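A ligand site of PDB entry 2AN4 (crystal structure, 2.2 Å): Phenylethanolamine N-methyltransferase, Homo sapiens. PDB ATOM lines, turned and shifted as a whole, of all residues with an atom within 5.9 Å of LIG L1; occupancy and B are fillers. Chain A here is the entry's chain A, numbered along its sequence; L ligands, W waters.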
ATOM      1  N   TYR A  35     -11.722  34.514 -32.383  1.00  0.00           N
ATOM      2  CA  TYR A  35     -12.146  33.774 -31.209  1.00  0.00           C
ATOM      3  C   TYR A  35     -13.089  34.653 -30.382  1.00  0.00           C
ATOM      4  O   TYR A  35     -14.186  34.231 -30.020  1.00  0.00           O
ATOM      5  CB  TYR A  35     -10.925  33.374 -30.360  1.00  0.00           C
ATOM      6  CG  TYR A  35     -11.305  32.647 -29.097  1.00  0.00           C
ATOM      7  CD1 TYR A  35     -11.790  31.332 -29.144  1.00  0.00           C
ATOM      8  CD2 TYR A  35     -11.225  33.278 -27.854  1.00  0.00           C
ATOM      9  CE1 TYR A  35     -12.180  30.663 -27.973  1.00  0.00           C
ATOM     10  CE2 TYR A  35     -11.611  32.624 -26.687  1.00  0.00           C
ATOM     11  CZ  TYR A  35     -12.084  31.321 -26.750  1.00  0.00           C
ATOM     12  OH  TYR A  35     -12.426  30.653 -25.610  1.00  0.00           O
ATOM     13  N   ASN A  39     -17.190  33.958 -29.522  1.00  0.00           N
ATOM     14  CA  ASN A  39     -17.660  33.632 -28.194  1.00  0.00           C
ATOM     15  C   ASN A  39     -17.923  34.764 -27.229  1.00  0.00           C
ATOM     16  O   ASN A  39     -18.464  34.522 -26.158  1.00  0.00           O
ATOM     17  CB  ASN A  39     -16.658  32.666 -27.560  1.00  0.00           C
ATOM     18  CG  ASN A  39     -16.462  31.421 -28.404  1.00  0.00           C
ATOM     19  OD1 ASN A  39     -17.329  30.559 -28.464  1.00  0.00           O
ATOM     20  ND2 ASN A  39     -15.316  31.335 -29.066  1.00  0.00           N
ATOM     21  N   TYR A  40     -17.542  35.985 -27.587  1.00  0.00           N
ATOM     22  CA  TYR A  40     -17.777  37.086 -26.679  1.00  0.00           C
ATOM     23  C   TYR A  40     -18.452  38.309 -27.281  1.00  0.00           C
ATOM     24  O   TYR A  40     -18.406  39.404 -26.733  1.00  0.00           O
ATOM     25  CB  TYR A  40     -16.454  37.435 -25.989  1.00  0.00           C
ATOM     26  CG  TYR A  40     -15.964  36.249 -25.191  1.00  0.00           C
ATOM     27  CD1 TYR A  40     -15.072  35.337 -25.750  1.00  0.00           C
ATOM     28  CD2 TYR A  40     -16.463  35.985 -23.914  1.00  0.00           C
ATOM     29  CE1 TYR A  40     -14.697  34.167 -25.056  1.00  0.00           C
ATOM     30  CE2 TYR A  40     -16.091  34.836 -23.214  1.00  0.00           C
ATOM     31  CZ  TYR A  40     -15.216  33.939 -23.783  1.00  0.00           C
ATOM     32  OH  TYR A  40     -14.876  32.805 -23.084  1.00  0.00           O
ATOM     33  N   ARG A  44     -23.720  35.087 -27.958  1.00  0.00           N
ATOM     34  CA  ARG A  44     -23.136  34.654 -26.687  1.00  0.00           C
ATOM     35  C   ARG A  44     -22.640  35.853 -25.883  1.00  0.00           C
ATOM     36  O   ARG A  44     -22.595  35.823 -24.653  1.00  0.00           O
ATOM     37  CB  ARG A  44     -21.969  33.685 -26.928  1.00  0.00           C
ATOM     38  CG  ARG A  44     -22.395  32.398 -27.596  1.00  0.00           C
ATOM     39  CD  ARG A  44     -21.241  31.419 -27.757  1.00  0.00           C
ATOM     40  NE  ARG A  44     -21.725  30.216 -28.432  1.00  0.00           N
ATOM     41  CZ  ARG A  44     -21.005  29.110 -28.672  1.00  0.00           C
ATOM     42  NH1 ARG A  44     -19.727  29.028 -28.310  1.00  0.00           N
ATOM     43  NH2 ARG A  44     -21.585  28.086 -29.278  1.00  0.00           N
ATOM     44  N   VAL A  53     -24.971  32.117 -21.554  1.00  0.00           N
ATOM     45  CA  VAL A  53     -23.767  31.485 -21.028  1.00  0.00           C
ATOM     46  C   VAL A  53     -22.810  32.491 -20.358  1.00  0.00           C
ATOM     47  O   VAL A  53     -22.046  32.143 -19.451  1.00  0.00           O
ATOM     48  CB  VAL A  53     -23.002  30.710 -22.149  1.00  0.00           C
ATOM     49  CG1 VAL A  53     -22.681  31.648 -23.325  1.00  0.00           C
ATOM     50  CG2 VAL A  53     -21.716  30.074 -21.575  1.00  0.00           C
ATOM     51  N   LYS A  57     -21.462  32.209 -16.418  1.00  0.00           N
ATOM     52  CA  LYS A  57     -20.066  32.140 -16.037  1.00  0.00           C
ATOM     53  C   LYS A  57     -19.676  33.250 -15.048  1.00  0.00           C
ATOM     54  O   LYS A  57     -18.944  33.006 -14.093  1.00  0.00           O
ATOM     55  CB  LYS A  57     -19.174  32.197 -17.286  1.00  0.00           C
ATOM     56  CG  LYS A  57     -19.329  30.986 -18.193  1.00  0.00           C
ATOM     57  CD  LYS A  57     -18.362  30.996 -19.376  1.00  0.00           C
ATOM     58  CE  LYS A  57     -18.562  32.232 -20.269  1.00  0.00           C
ATOM     59  NZ  LYS A  57     -17.746  32.166 -21.518  1.00  0.00           N
ATOM     60  N   PHE A 182     -11.492  27.291 -20.365  1.00  0.00           N
ATOM     61  CA  PHE A 182     -11.395  26.722 -21.712  1.00  0.00           C
ATOM     62  C   PHE A 182      -9.974  26.525 -22.223  1.00  0.00           C
ATOM     63  O   PHE A 182      -9.670  26.807 -23.374  1.00  0.00           O
ATOM     64  CB  PHE A 182     -12.181  27.602 -22.702  1.00  0.00           C
ATOM     65  CG  PHE A 182     -13.586  27.840 -22.293  1.00  0.00           C
ATOM     66  CD1 PHE A 182     -13.931  29.004 -21.603  1.00  0.00           C
ATOM     67  CD2 PHE A 182     -14.571  26.885 -22.536  1.00  0.00           C
ATOM     68  CE1 PHE A 182     -15.237  29.206 -21.174  1.00  0.00           C
ATOM     69  CE2 PHE A 182     -15.878  27.087 -22.107  1.00  0.00           C
ATOM     70  CZ  PHE A 182     -16.207  28.250 -21.424  1.00  0.00           C
ATOM     71  N   GLU A 185      -8.925  21.305 -21.713  1.00  0.00           N
ATOM     72  CA  GLU A 185      -9.601  20.465 -22.688  1.00  0.00           C
ATOM     73  C   GLU A 185      -9.393  20.916 -24.127  1.00  0.00           C
ATOM     74  O   GLU A 185      -9.550  20.143 -25.058  1.00  0.00           O
ATOM     75  CB  GLU A 185     -11.105  20.387 -22.367  1.00  0.00           C
ATOM     76  CG  GLU A 185     -11.933  21.580 -22.818  1.00  0.00           C
ATOM     77  CD  GLU A 185     -11.898  22.736 -21.836  1.00  0.00           C
ATOM     78  OE1 GLU A 185     -11.102  22.689 -20.870  1.00  0.00           O
ATOM     79  OE2 GLU A 185     -12.670  23.694 -22.050  1.00  0.00           O
ATOM     80  N   ALA A 186      -9.014  22.189 -24.309  1.00  0.00           N
ATOM     81  CA  ALA A 186      -8.794  22.706 -25.661  1.00  0.00           C
ATOM     82  C   ALA A 186      -7.368  22.508 -26.149  1.00  0.00           C
ATOM     83  O   ALA A 186      -7.059  22.817 -27.291  1.00  0.00           O
ATOM     84  CB  ALA A 186      -9.158  24.193 -25.707  1.00  0.00           C
ATOM     85  N   ALA A 216     -15.327  23.549 -21.535  1.00  0.00           N
ATOM     86  CA  ALA A 216     -16.363  23.048 -22.415  1.00  0.00           C
ATOM     87  C   ALA A 216     -16.716  21.590 -22.116  1.00  0.00           C
ATOM     88  O   ALA A 216     -15.822  20.752 -21.924  1.00  0.00           O
ATOM     89  CB  ALA A 216     -15.921  23.196 -23.869  1.00  0.00           C
ATOM     90  N   GLU A 219     -17.392  18.732 -25.911  1.00  0.00           N
ATOM     91  CA  GLU A 219     -17.086  19.474 -27.130  1.00  0.00           C
ATOM     92  C   GLU A 219     -15.895  18.796 -27.831  1.00  0.00           C
ATOM     93  O   GLU A 219     -15.047  18.197 -27.167  1.00  0.00           O
ATOM     94  CB  GLU A 219     -16.725  20.937 -26.806  1.00  0.00           C
ATOM     95  CG  GLU A 219     -16.104  21.699 -27.985  1.00  0.00           C
ATOM     96  CD  GLU A 219     -15.736  23.156 -27.672  1.00  0.00           C
ATOM     97  OE1 GLU A 219     -16.527  24.071 -27.989  1.00  0.00           O
ATOM     98  OE2 GLU A 219     -14.653  23.367 -27.098  1.00  0.00           O
ATOM     99  N   TRP A 221     -14.533  20.302 -31.143  1.00  0.00           N
ATOM    100  CA  TRP A 221     -13.869  21.269 -32.024  1.00  0.00           C
ATOM    101  C   TRP A 221     -14.489  22.645 -31.849  1.00  0.00           C
ATOM    102  O   TRP A 221     -15.623  22.762 -31.388  1.00  0.00           O
ATOM    103  CB  TRP A 221     -14.023  20.860 -33.501  1.00  0.00           C
ATOM    104  CG  TRP A 221     -15.457  20.832 -33.953  1.00  0.00           C
ATOM    105  CD1 TRP A 221     -16.327  19.774 -33.872  1.00  0.00           C
ATOM    106  CD2 TRP A 221     -16.222  21.919 -34.531  1.00  0.00           C
ATOM    107  NE1 TRP A 221     -17.570  20.130 -34.354  1.00  0.00           N
ATOM    108  CE2 TRP A 221     -17.527  21.441 -34.765  1.00  0.00           C
ATOM    109  CE3 TRP A 221     -15.911  23.248 -34.869  1.00  0.00           C
ATOM    110  CZ2 TRP A 221     -18.529  22.238 -35.335  1.00  0.00           C
ATOM    111  CZ3 TRP A 221     -16.915  24.042 -35.430  1.00  0.00           C
ATOM    112  CH2 TRP A 221     -18.206  23.536 -35.659  1.00  0.00           C
ATOM    113  N   TYR A 222     -13.737  23.675 -32.210  1.00  0.00           N
ATOM    114  CA  TYR A 222     -14.216  25.046 -32.167  1.00  0.00           C
ATOM    115  C   TYR A 222     -13.294  25.806 -33.112  1.00  0.00           C
ATOM    116  O   TYR A 222     -12.105  25.465 -33.257  1.00  0.00           O
ATOM    117  CB  TYR A 222     -14.189  25.621 -30.738  1.00  0.00           C
ATOM    118  CG  TYR A 222     -12.838  26.053 -30.210  1.00  0.00           C
ATOM    119  CD1 TYR A 222     -12.330  27.320 -30.493  1.00  0.00           C
ATOM    120  CD2 TYR A 222     -12.066  25.180 -29.444  1.00  0.00           C
ATOM    121  CE1 TYR A 222     -11.077  27.712 -30.030  1.00  0.00           C
ATOM    122  CE2 TYR A 222     -10.801  25.565 -28.970  1.00  0.00           C
ATOM    123  CZ  TYR A 222     -10.322  26.826 -29.262  1.00  0.00           C
ATOM    124  OH  TYR A 222      -9.083  27.210 -28.814  1.00  0.00           O
ATOM    125  N   VAL A 231     -10.793  19.326 -29.579  1.00  0.00           N
ATOM    126  CA  VAL A 231     -11.073  19.423 -28.153  1.00  0.00           C
ATOM    127  C   VAL A 231     -11.399  18.022 -27.670  1.00  0.00           C
ATOM    128  O   VAL A 231     -11.992  17.229 -28.399  1.00  0.00           O
ATOM    129  CB  VAL A 231     -12.301  20.345 -27.876  1.00  0.00           C
ATOM    130  CG1 VAL A 231     -12.514  20.517 -26.358  1.00  0.00           C
ATOM    131  CG2 VAL A 231     -12.112  21.688 -28.546  1.00  0.00           C
ATOM    132  N   MET A 258     -25.816  24.288 -22.975  1.00  0.00           N
ATOM    133  CA  MET A 258     -25.826  25.300 -24.016  1.00  0.00           C
ATOM    134  C   MET A 258     -27.168  25.328 -24.719  1.00  0.00           C
ATOM    135  O   MET A 258     -27.522  24.388 -25.433  1.00  0.00           O
ATOM    136  CB  MET A 258     -24.699  25.045 -25.024  1.00  0.00           C
ATOM    137  CG  MET A 258     -24.340  26.259 -25.902  1.00  0.00           C
ATOM    138  SD  MET A 258     -23.759  27.736 -24.981  1.00  0.00           S
ATOM    139  CE  MET A 258     -21.966  27.419 -24.798  1.00  0.00           C
ATOM    140  N   VAL A 266     -19.817  27.582 -34.498  1.00  0.00           N
ATOM    141  CA  VAL A 266     -18.430  28.012 -34.304  1.00  0.00           C
ATOM    142  C   VAL A 266     -17.779  26.874 -33.520  1.00  0.00           C
ATOM    143  O   VAL A 266     -16.578  26.859 -33.282  1.00  0.00           O
ATOM    144  CB  VAL A 266     -18.307  29.324 -33.468  1.00  0.00           C
ATOM    145  CG1 VAL A 266     -19.017  30.446 -34.173  1.00  0.00           C
ATOM    146  CG2 VAL A 266     -18.839  29.113 -32.064  1.00  0.00           C
ATOM    147  N   ASP A 267     -18.626  25.930 -33.110  1.00  0.00           N
ATOM    148  CA  ASP A 267     -18.194  24.752 -32.363  1.00  0.00           C
ATOM    149  C   ASP A 267     -19.375  23.804 -32.217  1.00  0.00           C
ATOM    150  O   ASP A 267     -20.431  24.027 -32.819  1.00  0.00           O
ATOM    151  CB  ASP A 267     -17.687  25.143 -30.977  1.00  0.00           C
ATOM    152  CG  ASP A 267     -18.718  25.904 -30.153  1.00  0.00           C
ATOM    153  OD1 ASP A 267     -19.908  25.509 -30.154  1.00  0.00           O
ATOM    154  OD2 ASP A 267     -18.338  26.896 -29.491  1.00  0.00           O
ATOM    155  N   VAL A 269     -20.001  22.565 -28.900  1.00  0.00           N
ATOM    156  CA  VAL A 269     -20.071  22.491 -27.440  1.00  0.00           C
ATOM    157  C   VAL A 269     -21.491  22.127 -26.968  1.00  0.00           C
ATOM    158  O   VAL A 269     -22.478  22.607 -27.539  1.00  0.00           O
ATOM    159  CB  VAL A 269     -19.611  23.841 -26.799  1.00  0.00           C
ATOM    160  CG1 VAL A 269     -20.585  24.951 -27.190  1.00  0.00           C
ATOM    161  CG2 VAL A 269     -19.502  23.708 -25.299  1.00  0.00           C
ATOM    162  N   VAL A 272     -21.246  23.732 -20.418  1.00  0.00           N
ATOM    163  CA  VAL A 272     -20.085  24.418 -19.849  1.00  0.00           C
ATOM    164  C   VAL A 272     -20.038  24.066 -18.367  1.00  0.00           C
ATOM    165  O   VAL A 272     -21.077  24.062 -17.689  1.00  0.00           O
ATOM    166  CB  VAL A 272     -20.205  25.956 -20.031  1.00  0.00           C
ATOM    167  CG1 VAL A 272     -19.126  26.670 -19.235  1.00  0.00           C
ATOM    168  CG2 VAL A 272     -20.091  26.315 -21.498  1.00  0.00           C
HETATM  169  C1  LIG L   1     -17.648  27.594 -25.809  1.00  0.00           C
HETATM  170  C2  LIG L   1     -18.632  28.464 -25.357  1.00  0.00           C
HETATM  171  C3  LIG L   1     -18.285  29.720 -24.876  1.00  0.00           C
HETATM  172  O1  LIG L   1     -19.251  30.568 -24.439  1.00  0.00           O
HETATM  173  C4  LIG L   1     -16.943  30.099 -24.836  1.00  0.00           C
HETATM  174  C5  LIG L   1     -15.961  29.216 -25.293  1.00  0.00           C
HETATM  175  C6  LIG L   1     -16.308  27.960 -25.773  1.00  0.00           C
HETATM  176  C7  LIG L   1     -15.260  26.971 -26.270  1.00  0.00           C
HETATM  177  O2  LIG L   1     -15.347  26.851 -27.696  1.00  0.00           O
HETATM  178  C8  LIG L   1     -13.839  27.402 -25.887  1.00  0.00           C
HETATM  179  N1  LIG L   1     -12.861  26.417 -26.398  1.00  0.00           N
HETATM  180  N1  LG2 L   2      -9.306  31.520 -21.381  1.00  0.00           N
HETATM  181  C1  LG2 L   2      -9.979  32.172 -22.505  1.00  0.00           C
HETATM  182  C2  LG2 L   2      -9.350  31.673 -23.845  1.00  0.00           C
HETATM  183  C3  LG2 L   2      -9.288  30.141 -24.049  1.00  0.00           C
HETATM  184  S1  LG2 L   2      -8.759  29.675 -25.742  1.00  0.00           S
HETATM  185  C4  LG2 L   2     -11.500  31.990 -22.478  1.00  0.00           C
HETATM  186  O1  LG2 L   2     -12.155  32.049 -23.539  1.00  0.00           O
HETATM  187  O2  LG2 L   2     -12.056  31.827 -21.363  1.00  0.00           O
HETATM  188  C5  LG2 L   2      -7.479  28.429 -25.426  1.00  0.00           C
HETATM  189  C6  LG2 L   2      -6.124  29.077 -25.288  1.00  0.00           C
HETATM  190  O3  LG2 L   2      -5.094  28.125 -24.900  1.00  0.00           O
HETATM  191  C7  LG2 L   2      -5.588  29.836 -26.497  1.00  0.00           C
HETATM  192  O4  LG2 L   2      -5.331  31.191 -26.154  1.00  0.00           O
HETATM  193  C8  LG2 L   2      -4.333  29.049 -26.887  1.00  0.00           C
HETATM  194  O5  LG2 L   2      -3.308  29.816 -27.486  1.00  0.00           O
HETATM  195  C9  LG2 L   2      -3.889  28.485 -25.537  1.00  0.00           C
HETATM  196  N2  LG2 L   2      -3.001  27.316 -25.611  1.00  0.00           N
HETATM  197  C10 LG2 L   2      -2.691  26.485 -26.739  1.00  0.00           C
HETATM  198  N3  LG2 L   2      -1.792  25.564 -26.465  1.00  0.00           N
HETATM  199  C11 LG2 L   2      -1.528  25.765 -25.115  1.00  0.00           C
HETATM  200  C12 LG2 L   2      -0.620  25.078 -24.285  1.00  0.00           C
HETATM  201  N4  LG2 L   2       0.154  24.073 -24.684  1.00  0.00           N
HETATM  202  N5  LG2 L   2      -0.532  25.487 -22.981  1.00  0.00           N
HETATM  203  C13 LG2 L   2      -1.313  26.522 -22.574  1.00  0.00           C
HETATM  204  N6  LG2 L   2      -2.203  27.249 -23.292  1.00  0.00           N
HETATM  205  C14 LG2 L   2      -2.258  26.811 -24.576  1.00  0.00           C
HETATM  206  O   HOH W   1     -16.112  28.130 -29.636  1.00  0.00           O
HETATM  207  O   HOH W   2     -12.817  24.229 -24.940  1.00  0.00           O
HETATM  208  O   HOH W   3     -18.800  33.145 -23.861  1.00  0.00           O
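OD2 of Asp 267 is in hydrogen-bond range of O2 of LIG L1, 3.5 Å away. An oxygen (O1) of LG2 L2 lies within hydrogen-bond range of the side-chain hydroxyl (OH) of Tyr 40. An oxygen (O1) of LG2 L2 is in hydrogen-bond range of the side-chain hydroxyl (OH) of Tyr 35 (2.5 Å). A nitrogen (N1) of LIG L1 is in salt-bridge range of the side-chain carboxylate (OE2) of Glu 219, at 3.6 Å.
OD2 of Asp 267 lies within salt-bridge range of NH1 of Arg 44. The side-chain amide nitrogen (ND2) of Asn 39 sits at hydrogen-bond distance from the backbone carbonyl oxygen (O) of Tyr 35. NH1 of Arg 44 lies within hydrogen-bond range of OD1 of Asn 39 (2.8 Å). OH of Tyr 40 lies within hydrogen-bond range of NZ of Lys 57 (3.3 Å). OD1 of Asp 267 sits close to N of Val 269 (3.2 Å).
Residues that only touch LIG L1: Arg 44 (3.2 Å), Tyr 222 (3.4 Å), Phe 182 (3.5 Å), Met 258 (3.5 Å), Tyr 35 (3.6 Å), Lys 57 (3.7 Å), Asn 39 (3.7 Å), Val 53 (3.8 Å) and Tyr 40 (3.8 Å). Of the 19 residues printed, 11 come within 4 Å of LIG L1. The nearest printed residue that does not touch LIG L1 is Val 269 (4.2 Å).
Water W1 lies within hydrogen-bond range of O2 of LIG L1 (2.4 Å), OD2 of Asp 267 (2.5 Å) and OD1 of Asn 39 (3.0 Å). Water W2 lies within hydrogen-bond range of a nitrogen (N1) of LIG L1, the side-chain carboxylate (OE2) of Glu 185 and the side-chain carboxylate (OE2) of Glu 219. Water W3 lies within hydrogen-bond range of O1 of LIG L1, O of Asn 39 and NZ of Lys 57.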
